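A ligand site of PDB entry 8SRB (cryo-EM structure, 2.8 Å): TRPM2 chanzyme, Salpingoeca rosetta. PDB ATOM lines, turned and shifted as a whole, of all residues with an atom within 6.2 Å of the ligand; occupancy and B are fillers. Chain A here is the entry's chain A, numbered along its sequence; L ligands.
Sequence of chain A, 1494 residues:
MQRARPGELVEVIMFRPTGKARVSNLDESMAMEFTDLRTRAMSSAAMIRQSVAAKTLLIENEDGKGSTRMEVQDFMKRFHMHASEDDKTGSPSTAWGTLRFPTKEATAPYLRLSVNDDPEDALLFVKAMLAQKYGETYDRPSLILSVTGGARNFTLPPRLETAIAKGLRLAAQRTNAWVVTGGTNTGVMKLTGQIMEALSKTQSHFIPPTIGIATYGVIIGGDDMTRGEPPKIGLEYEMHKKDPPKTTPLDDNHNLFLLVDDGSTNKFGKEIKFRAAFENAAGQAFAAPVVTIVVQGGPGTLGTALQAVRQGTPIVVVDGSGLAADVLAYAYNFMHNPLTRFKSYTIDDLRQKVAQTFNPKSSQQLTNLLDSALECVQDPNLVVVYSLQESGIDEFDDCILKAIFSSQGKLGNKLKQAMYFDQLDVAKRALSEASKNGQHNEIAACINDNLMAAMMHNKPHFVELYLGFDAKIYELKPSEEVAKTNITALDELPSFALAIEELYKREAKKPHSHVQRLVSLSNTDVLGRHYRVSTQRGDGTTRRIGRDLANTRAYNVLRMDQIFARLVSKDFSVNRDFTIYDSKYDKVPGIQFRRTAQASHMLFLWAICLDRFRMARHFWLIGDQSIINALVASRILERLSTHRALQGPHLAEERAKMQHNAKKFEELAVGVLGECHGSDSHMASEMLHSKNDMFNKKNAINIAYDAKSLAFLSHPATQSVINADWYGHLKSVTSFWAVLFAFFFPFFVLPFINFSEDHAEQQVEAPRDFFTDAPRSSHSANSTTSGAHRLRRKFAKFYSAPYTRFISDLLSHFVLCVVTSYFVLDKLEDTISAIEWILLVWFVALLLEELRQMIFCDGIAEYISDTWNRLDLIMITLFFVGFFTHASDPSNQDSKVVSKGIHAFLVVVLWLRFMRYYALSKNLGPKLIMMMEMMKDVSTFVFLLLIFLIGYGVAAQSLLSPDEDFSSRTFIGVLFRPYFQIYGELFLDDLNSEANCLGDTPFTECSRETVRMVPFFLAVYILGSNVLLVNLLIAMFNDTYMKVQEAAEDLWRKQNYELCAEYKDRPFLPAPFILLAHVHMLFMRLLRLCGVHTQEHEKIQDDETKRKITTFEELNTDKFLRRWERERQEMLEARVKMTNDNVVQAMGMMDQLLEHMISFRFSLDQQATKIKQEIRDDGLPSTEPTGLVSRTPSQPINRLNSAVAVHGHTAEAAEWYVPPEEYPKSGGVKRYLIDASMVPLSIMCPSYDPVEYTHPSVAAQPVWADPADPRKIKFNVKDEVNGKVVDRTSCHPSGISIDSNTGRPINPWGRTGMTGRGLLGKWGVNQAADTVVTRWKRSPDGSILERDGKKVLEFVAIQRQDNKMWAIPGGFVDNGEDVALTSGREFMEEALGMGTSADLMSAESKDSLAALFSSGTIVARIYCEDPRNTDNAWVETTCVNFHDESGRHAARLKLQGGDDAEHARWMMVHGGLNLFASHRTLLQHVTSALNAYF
An oxygen (O12) of the ligand sits at hydrogen-bond distance from the backbone NH of Gly 149, at 2.9 Å. The backbone carbonyl oxygen of Gly 149 sits at hydrogen-bond distance from an oxygen (O12) of the ligand, 2.7 Å away. N of Ala 151 lies within hydrogen-bond range of O5 of the ligand (2.8 Å). O12 of the ligand is in hydrogen-bond range of OG1 of Thr 148. The side-chain hydroxyl (OG1) of Thr 184 is in hydrogen-bond range of a nitrogen (N1) of the ligand, at 3.0 Å. NH1 of Arg 275 lies within hydrogen-bond range of O13 of the ligand (3.1 Å). The backbone NH (N) of Gly 298 sits at hydrogen-bond distance from an oxygen (O9) of the ligand, 3.2 Å away. N of Arg 152 sits at hydrogen-bond distance from O5 of the ligand (3.3 Å). N of Gly 300 lies within hydrogen-bond range of O8 of the ligand, at 3.4 Å.
O of Ala 151 is in hydrogen-bond range of OG1 of Thr 186, at 2.6 Å. The backbone carbonyl oxygen (O) of Val 147 is in hydrogen-bond range of the guanidinium group (NH2) of Arg 275 (2.6 Å). The side-chain hydroxyl of Thr 301 sits at hydrogen-bond distance from the backbone NH of Gly 298 (3.0 Å). O of Gly 300 is in hydrogen-bond range of OG1 of Thr 304 (2.7 Å). The backbone NH (N) of Val 188 sits at hydrogen-bond distance from the backbone carbonyl oxygen (O) of Gly 150, at 3.2 Å.
The backbone nitrogen of Pro 299 lies close to an oxygen (O8) of the ligand, at 3.4 Å. C of Gly 150 touches O5 of the ligand (3.8 Å). Met 189 touches the ligand. Phe 268 touches the ligand. CG1 of Ile 272 touches O14 of the ligand (3.7 Å). Thr 301 touches the ligand. Hydrophobic or aromatic side chains that line the ligand: Ala 151, Met 189, Phe 268, Ile 272 and Pro 299. Within 4 Å of the ligand: Thr 148, Gly 149, Gly 150, Ala 151, Arg 152, Thr 184, Met 189, Phe 268, Ile 272, Arg 275, Gly 298, Pro 299, Gly 300 and Thr 301.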
ATOM      1  N   VAL A 147       0.717   3.032  11.869  1.00  0.00           N
ATOM      2  CA  VAL A 147       1.378   3.526  10.631  1.00  0.00           C
ATOM      3  C   VAL A 147       0.706   4.833  10.256  1.00  0.00           C
ATOM      4  O   VAL A 147      -0.509   4.839  10.077  1.00  0.00           O
ATOM      5  CB  VAL A 147       1.278   2.516   9.479  1.00  0.00           C
ATOM      6  CG1 VAL A 147       2.039   3.003   8.258  1.00  0.00           C
ATOM      7  CG2 VAL A 147       1.770   1.144   9.891  1.00  0.00           C
ATOM      8  N   THR A 148       1.490   5.894  10.101  1.00  0.00           N
ATOM      9  CA  THR A 148       0.898   7.211   9.806  1.00  0.00           C
ATOM     10  C   THR A 148       1.702   7.906   8.718  1.00  0.00           C
ATOM     11  O   THR A 148       2.933   7.801   8.750  1.00  0.00           O
ATOM     12  CB  THR A 148       0.808   8.076  11.067  1.00  0.00           C
ATOM     13  OG1 THR A 148       0.040   9.223  10.713  1.00  0.00           O
ATOM     14  CG2 THR A 148       2.153   8.526  11.602  1.00  0.00           C
ATOM     15  N   GLY A 149       1.023   8.505   7.762  1.00  0.00           N
ATOM     16  CA  GLY A 149       1.652   9.288   6.729  1.00  0.00           C
ATOM     17  C   GLY A 149       0.633   9.907   5.796  1.00  0.00           C
ATOM     18  O   GLY A 149      -0.455  10.288   6.230  1.00  0.00           O
ATOM     19  N   GLY A 150       1.058  10.039   4.535  1.00  0.00           N
ATOM     20  CA  GLY A 150       0.297  10.785   3.537  1.00  0.00           C
ATOM     21  C   GLY A 150      -1.020  10.163   3.127  1.00  0.00           C
ATOM     22  O   GLY A 150      -1.088   9.007   2.715  1.00  0.00           O
ATOM     23  N   ALA A 151      -2.068  10.965   3.215  1.00  0.00           N
ATOM     24  CA  ALA A 151      -3.370  10.546   2.730  1.00  0.00           C
ATOM     25  C   ALA A 151      -3.454  10.575   1.219  1.00  0.00           C
ATOM     26  O   ALA A 151      -3.918   9.607   0.619  1.00  0.00           O
ATOM     27  CB  ALA A 151      -4.447  11.403   3.347  1.00  0.00           C
ATOM     28  N   ARG A 152      -2.924  11.628   0.581  1.00  0.00           N
ATOM     29  CA  ARG A 152      -2.976  11.783  -0.861  1.00  0.00           C
ATOM     30  C   ARG A 152      -2.009  10.831  -1.565  1.00  0.00           C
ATOM     31  O   ARG A 152      -1.108  10.273  -0.934  1.00  0.00           O
ATOM     32  CB  ARG A 152      -2.657  13.227  -1.259  1.00  0.00           C
ATOM     33  N   THR A 181      -3.764   2.043  11.302  1.00  0.00           N
ATOM     34  CA  THR A 181      -3.649   3.100  10.302  1.00  0.00           C
ATOM     35  C   THR A 181      -4.967   3.860  10.268  1.00  0.00           C
ATOM     36  O   THR A 181      -5.818   3.664  11.132  1.00  0.00           O
ATOM     37  CB  THR A 181      -3.397   2.594   8.870  1.00  0.00           C
ATOM     38  OG1 THR A 181      -4.632   2.166   8.295  1.00  0.00           O
ATOM     39  CG2 THR A 181      -2.381   1.510   8.772  1.00  0.00           C
ATOM     40  N   GLY A 182      -5.107   4.770   9.311  1.00  0.00           N
ATOM     41  CA  GLY A 182      -6.378   5.495   9.145  1.00  0.00           C
ATOM     42  C   GLY A 182      -7.354   4.612   8.369  1.00  0.00           C
ATOM     43  O   GLY A 182      -7.054   3.421   8.219  1.00  0.00           O
ATOM     44  N   GLY A 183      -8.475   5.139   7.901  1.00  0.00           N
ATOM     45  CA  GLY A 183      -9.449   4.256   7.246  1.00  0.00           C
ATOM     46  C   GLY A 183      -9.662   4.601   5.788  1.00  0.00           C
ATOM     47  O   GLY A 183     -10.293   3.811   5.080  1.00  0.00           O
ATOM     48  N   THR A 184      -9.132   5.738   5.361  1.00  0.00           N
ATOM     49  CA  THR A 184      -9.409   6.183   3.969  1.00  0.00           C
ATOM     50  C   THR A 184      -8.704   5.227   3.008  1.00  0.00           C
ATOM     51  O   THR A 184      -7.774   4.555   3.437  1.00  0.00           O
ATOM     52  CB  THR A 184      -9.098   7.661   3.803  1.00  0.00           C
ATOM     53  OG1 THR A 184      -9.419   8.288   5.039  1.00  0.00           O
ATOM     54  CG2 THR A 184      -9.895   8.312   2.693  1.00  0.00           C
ATOM     55  N   THR A 186      -6.992   6.013   0.436  1.00  0.00           N
ATOM     56  CA  THR A 186      -5.973   6.673  -0.403  1.00  0.00           C
ATOM     57  C   THR A 186      -4.612   6.715   0.282  1.00  0.00           C
ATOM     58  O   THR A 186      -4.581   6.853   1.512  1.00  0.00           O
ATOM     59  CB  THR A 186      -6.443   8.070  -0.829  1.00  0.00           C
ATOM     60  OG1 THR A 186      -5.338   8.760  -1.425  1.00  0.00           O
ATOM     61  CG2 THR A 186      -7.026   8.881   0.302  1.00  0.00           C
ATOM     62  N   VAL A 188      -1.140   5.897   2.108  1.00  0.00           N
ATOM     63  CA  VAL A 188      -0.498   4.851   2.965  1.00  0.00           C
ATOM     64  C   VAL A 188      -1.526   3.786   3.323  1.00  0.00           C
ATOM     65  O   VAL A 188      -1.251   2.601   3.101  1.00  0.00           O
ATOM     66  CB  VAL A 188       0.139   5.499   4.207  1.00  0.00           C
ATOM     67  CG1 VAL A 188       0.702   4.475   5.181  1.00  0.00           C
ATOM     68  CG2 VAL A 188       1.204   6.512   3.844  1.00  0.00           C
ATOM     69  N   MET A 189      -2.682   4.196   3.812  1.00  0.00           N
ATOM     70  CA  MET A 189      -3.698   3.242   4.253  1.00  0.00           C
ATOM     71  C   MET A 189      -3.998   2.184   3.187  1.00  0.00           C
ATOM     72  O   MET A 189      -4.099   0.992   3.504  1.00  0.00           O
ATOM     73  CB  MET A 189      -4.952   3.958   4.682  1.00  0.00           C
ATOM     74  CG  MET A 189      -4.758   5.024   5.709  1.00  0.00           C
ATOM     75  SD  MET A 189      -4.234   6.628   5.110  1.00  0.00           S
ATOM     76  CE  MET A 189      -5.756   7.376   4.616  1.00  0.00           C
ATOM     77  N   ILE A 213      -8.732   3.591  12.154  1.00  0.00           N
ATOM     78  CA  ILE A 213      -9.361   4.639  12.946  1.00  0.00           C
ATOM     79  C   ILE A 213      -9.462   5.902  12.118  1.00  0.00           C
ATOM     80  O   ILE A 213      -8.431   6.490  11.769  1.00  0.00           O
ATOM     81  CB  ILE A 213      -8.589   4.899  14.236  1.00  0.00           C
ATOM     82  CG1 ILE A 213      -8.435   3.580  15.003  1.00  0.00           C
ATOM     83  CG2 ILE A 213      -9.285   5.975  15.039  1.00  0.00           C
ATOM     84  CD1 ILE A 213      -7.718   3.719  16.300  1.00  0.00           C
ATOM     85  N   ALA A 214     -10.671   6.340  11.776  1.00  0.00           N
ATOM     86  CA  ALA A 214     -10.802   7.485  10.893  1.00  0.00           C
ATOM     87  C   ALA A 214     -11.803   8.436  11.532  1.00  0.00           C
ATOM     88  O   ALA A 214     -12.679   7.996  12.294  1.00  0.00           O
ATOM     89  CB  ALA A 214     -11.262   7.089   9.497  1.00  0.00           C
ATOM     90  N   THR A 215     -11.641   9.726  11.265  1.00  0.00           N
ATOM     91  CA  THR A 215     -12.634  10.682  11.734  1.00  0.00           C
ATOM     92  C   THR A 215     -13.956  10.608  10.966  1.00  0.00           C
ATOM     93  O   THR A 215     -13.966  10.464   9.730  1.00  0.00           O
ATOM     94  CB  THR A 215     -12.046  12.098  11.728  1.00  0.00           C
ATOM     95  OG1 THR A 215     -13.034  13.043  12.177  1.00  0.00           O
ATOM     96  CG2 THR A 215     -11.393  12.520  10.399  1.00  0.00           C
ATOM     97  N   VAL A 218     -16.331  12.416   7.166  1.00  0.00           N
ATOM     98  CA  VAL A 218     -15.684  12.467   5.865  1.00  0.00           C
ATOM     99  C   VAL A 218     -15.979  11.203   5.086  1.00  0.00           C
ATOM    100  O   VAL A 218     -15.669  11.139   3.909  1.00  0.00           O
ATOM    101  CB  VAL A 218     -14.163  12.688   5.972  1.00  0.00           C
ATOM    102  CG1 VAL A 218     -13.822  13.940   6.788  1.00  0.00           C
ATOM    103  CG2 VAL A 218     -13.467  11.469   6.523  1.00  0.00           C
ATOM    104  N   THR A 248     -14.587  11.178   0.692  1.00  0.00           N
ATOM    105  CA  THR A 248     -13.578  10.194   1.045  1.00  0.00           C
ATOM    106  C   THR A 248     -14.174   8.825   1.396  1.00  0.00           C
ATOM    107  O   THR A 248     -14.837   8.703   2.436  1.00  0.00           O
ATOM    108  CB  THR A 248     -12.768  10.763   2.210  1.00  0.00           C
ATOM    109  N   PHE A 268     -10.970  17.582   8.923  1.00  0.00           N
ATOM    110  CA  PHE A 268     -10.069  16.461   9.246  1.00  0.00           C
ATOM    111  C   PHE A 268      -9.230  16.743  10.481  1.00  0.00           C
ATOM    112  O   PHE A 268      -9.317  17.859  11.008  1.00  0.00           O
ATOM    113  CB  PHE A 268      -9.152  16.118   8.061  1.00  0.00           C
ATOM    114  CG  PHE A 268      -9.815  15.643   6.801  1.00  0.00           C
ATOM    115  CD1 PHE A 268     -10.300  16.553   5.867  1.00  0.00           C
ATOM    116  CD2 PHE A 268      -9.910  14.299   6.519  1.00  0.00           C
ATOM    117  CE1 PHE A 268     -10.885  16.109   4.694  1.00  0.00           C
ATOM    118  CE2 PHE A 268     -10.494  13.855   5.346  1.00  0.00           C
ATOM    119  CZ  PHE A 268     -10.990  14.758   4.433  1.00  0.00           C
ATOM    120  N   GLY A 269      -8.472  15.765  10.937  1.00  0.00           N
ATOM    121  CA  GLY A 269      -7.540  15.752  12.061  1.00  0.00           C
ATOM    122  C   GLY A 269      -8.101  15.678  13.458  1.00  0.00           C
ATOM    123  O   GLY A 269      -7.338  15.854  14.409  1.00  0.00           O
ATOM    124  N   ILE A 272      -6.838  12.178  15.708  1.00  0.00           N
ATOM    125  CA  ILE A 272      -5.400  11.946  15.934  1.00  0.00           C
ATOM    126  C   ILE A 272      -5.089  11.638  17.409  1.00  0.00           C
ATOM    127  O   ILE A 272      -4.390  10.665  17.715  1.00  0.00           O
ATOM    128  CB  ILE A 272      -4.604  13.156  15.409  1.00  0.00           C
ATOM    129  CG1 ILE A 272      -4.804  13.299  13.906  1.00  0.00           C
ATOM    130  CG2 ILE A 272      -3.120  13.089  15.768  1.00  0.00           C
ATOM    131  CD1 ILE A 272      -4.159  14.538  13.304  1.00  0.00           C
ATOM    132  N   ARG A 275      -6.559   8.338  18.623  1.00  0.00           N
ATOM    133  CA  ARG A 275      -5.751   7.275  18.036  1.00  0.00           C
ATOM    134  C   ARG A 275      -4.494   7.005  18.851  1.00  0.00           C
ATOM    135  O   ARG A 275      -4.210   5.854  19.159  1.00  0.00           O
ATOM    136  CB  ARG A 275      -5.354   7.631  16.607  1.00  0.00           C
ATOM    137  CG  ARG A 275      -4.550   6.588  15.877  1.00  0.00           C
ATOM    138  CD  ARG A 275      -4.199   7.081  14.508  1.00  0.00           C
ATOM    139  NE  ARG A 275      -3.098   6.322  13.932  1.00  0.00           N
ATOM    140  CZ  ARG A 275      -2.702   6.399  12.671  1.00  0.00           C
ATOM    141  NH1 ARG A 275      -3.299   7.205  11.813  1.00  0.00           N
ATOM    142  NH2 ARG A 275      -1.675   5.662  12.262  1.00  0.00           N
ATOM    143  N   GLN A 296       6.049   9.542   3.797  1.00  0.00           N
ATOM    144  CA  GLN A 296       5.639  10.839   3.198  1.00  0.00           C
ATOM    145  C   GLN A 296       5.012  11.671   4.306  1.00  0.00           C
ATOM    146  O   GLN A 296       5.723  12.006   5.259  1.00  0.00           O
ATOM    147  CB  GLN A 296       4.586  10.626   2.117  1.00  0.00           C
ATOM    148  CG  GLN A 296       4.211  11.891   1.357  1.00  0.00           C
ATOM    149  CD  GLN A 296       3.295  11.579   0.198  1.00  0.00           C
ATOM    150  OE1 GLN A 296       2.130  11.253   0.374  1.00  0.00           O
ATOM    151  NE2 GLN A 296       3.823  11.694  -1.010  1.00  0.00           N
ATOM    152  N   GLY A 297       3.745  12.033   4.161  1.00  0.00           N
ATOM    153  CA  GLY A 297       3.035  12.764   5.197  1.00  0.00           C
ATOM    154  C   GLY A 297       2.940  14.259   5.016  1.00  0.00           C
ATOM    155  O   GLY A 297       3.735  14.897   4.318  1.00  0.00           O
ATOM    156  N   GLY A 298       1.865  14.814   5.576  1.00  0.00           N
ATOM    157  CA  GLY A 298       1.595  16.234   5.588  1.00  0.00           C
ATOM    158  C   GLY A 298       1.831  16.856   6.964  1.00  0.00           C
ATOM    159  O   GLY A 298       2.612  16.311   7.746  1.00  0.00           O
ATOM    160  N   PRO A 299       1.250  18.052   7.218  1.00  0.00           N
ATOM    161  CA  PRO A 299       1.397  18.719   8.548  1.00  0.00           C
ATOM    162  C   PRO A 299       0.837  17.970   9.759  1.00  0.00           C
ATOM    163  O   PRO A 299       1.413  18.074  10.861  1.00  0.00           O
ATOM    164  CB  PRO A 299       0.640  20.041   8.346  1.00  0.00           C
ATOM    165  CG  PRO A 299       0.632  20.278   6.912  1.00  0.00           C
ATOM    166  CD  PRO A 299       0.553  18.936   6.262  1.00  0.00           C
ATOM    167  N   GLY A 300      -0.276  17.244   9.591  1.00  0.00           N
ATOM    168  CA  GLY A 300      -0.837  16.505  10.711  1.00  0.00           C
ATOM    169  C   GLY A 300      -0.040  15.278  11.074  1.00  0.00           C
ATOM    170  O   GLY A 300      -0.125  14.815  12.227  1.00  0.00           O
ATOM    171  N   THR A 301       0.696  14.707  10.107  1.00  0.00           N
ATOM    172  CA  THR A 301       1.610  13.603  10.381  1.00  0.00           C
ATOM    173  C   THR A 301       2.784  14.060  11.235  1.00  0.00           C
ATOM    174  O   THR A 301       3.307  13.273  12.041  1.00  0.00           O
ATOM    175  CB  THR A 301       2.076  13.008   9.064  1.00  0.00           C
ATOM    176  OG1 THR A 301       2.808  14.005   8.343  1.00  0.00           O
ATOM    177  CG2 THR A 301       0.860  12.646   8.284  1.00  0.00           C
ATOM    178  N   THR A 304       1.359  14.353  14.618  1.00  0.00           N
ATOM    179  CA  THR A 304       1.215  12.967  15.078  1.00  0.00           C
ATOM    180  C   THR A 304       2.540  12.417  15.618  1.00  0.00           C
ATOM    181  O   THR A 304       2.587  11.834  16.706  1.00  0.00           O
ATOM    182  CB  THR A 304       0.705  12.120  13.908  1.00  0.00           C
ATOM    183  OG1 THR A 304      -0.613  12.556  13.541  1.00  0.00           O
ATOM    184  CG2 THR A 304       0.626  10.632  14.245  1.00  0.00           C
HETATM  185  N1  LIG L   1      -7.616  10.657   4.726  1.00  0.00           N
HETATM  186  C1  LIG L   1      -7.923  11.361   3.626  1.00  0.00           C
HETATM  187  N2  LIG L   1      -7.739  12.678   3.522  1.00  0.00           N
HETATM  188  C2  LIG L   1      -7.232  13.380   4.553  1.00  0.00           C
HETATM  189  C3  LIG L   1      -6.885  12.686   5.796  1.00  0.00           C
HETATM  190  C4  LIG L   1      -7.112  11.225   5.823  1.00  0.00           C
HETATM  191  N3  LIG L   1      -6.810  10.502   6.924  1.00  0.00           N
HETATM  192  N4  LIG L   1      -6.422  13.605   6.644  1.00  0.00           N
HETATM  193  C5  LIG L   1      -6.461  14.801   6.004  1.00  0.00           C
HETATM  194  N5  LIG L   1      -6.956  14.654   4.765  1.00  0.00           N
HETATM  195  C6  LIG L   1      -7.149  15.743   3.788  1.00  0.00           C
HETATM  196  C7  LIG L   1      -6.297  16.905   4.235  1.00  0.00           C
HETATM  197  O1  LIG L   1      -7.116  18.050   4.417  1.00  0.00           O
HETATM  198  C8  LIG L   1      -5.295  17.131   3.121  1.00  0.00           C
HETATM  199  O2  LIG L   1      -5.463  18.435   2.580  1.00  0.00           O
HETATM  200  O3  LIG L   1      -6.683  15.294   2.519  1.00  0.00           O
HETATM  201  C9  LIG L   1      -5.586  16.081   2.062  1.00  0.00           C
HETATM  202  C10 LIG L   1      -4.372  15.202   1.875  1.00  0.00           C
HETATM  203  O4  LIG L   1      -3.286  15.918   2.445  1.00  0.00           O
HETATM  204  P1  LIG L   1      -2.262  15.164   3.424  1.00  0.00           P
HETATM  205  O5  LIG L   1      -2.150  13.741   2.953  1.00  0.00           O
HETATM  206  O6  LIG L   1      -1.033  16.013   3.530  1.00  0.00           O
HETATM  207  O7  LIG L   1      -3.006  15.202   4.833  1.00  0.00           O
HETATM  208  P2  LIG L   1      -2.110  15.004   6.150  1.00  0.00           P
HETATM  209  O8  LIG L   1      -1.626  16.348   6.602  1.00  0.00           O
HETATM  210  O9  LIG L   1      -1.148  13.881   5.874  1.00  0.00           O
HETATM  211  O10 LIG L   1      -3.163  14.501   7.233  1.00  0.00           O
HETATM  212  C11 LIG L   1      -2.692  13.815   8.381  1.00  0.00           C
HETATM  213  O11 LIG L   1      -2.753  11.464   7.809  1.00  0.00           O
HETATM  214  O12 LIG L   1      -1.653   9.505   8.467  1.00  0.00           O
HETATM  215  C12 LIG L   1      -2.870  10.249   8.543  1.00  0.00           C
HETATM  216  O13 LIG L   1      -4.187   9.826  10.506  1.00  0.00           O
HETATM  217  C13 LIG L   1      -3.126  10.632   9.977  1.00  0.00           C
HETATM  218  O14 LIG L   1      -4.936  12.130  10.350  1.00  0.00           O
HETATM  219  C14 LIG L   1      -3.573  12.068   9.947  1.00  0.00           C
HETATM  220  C15 LIG L   1      -3.445  12.507   8.493  1.00  0.00           C
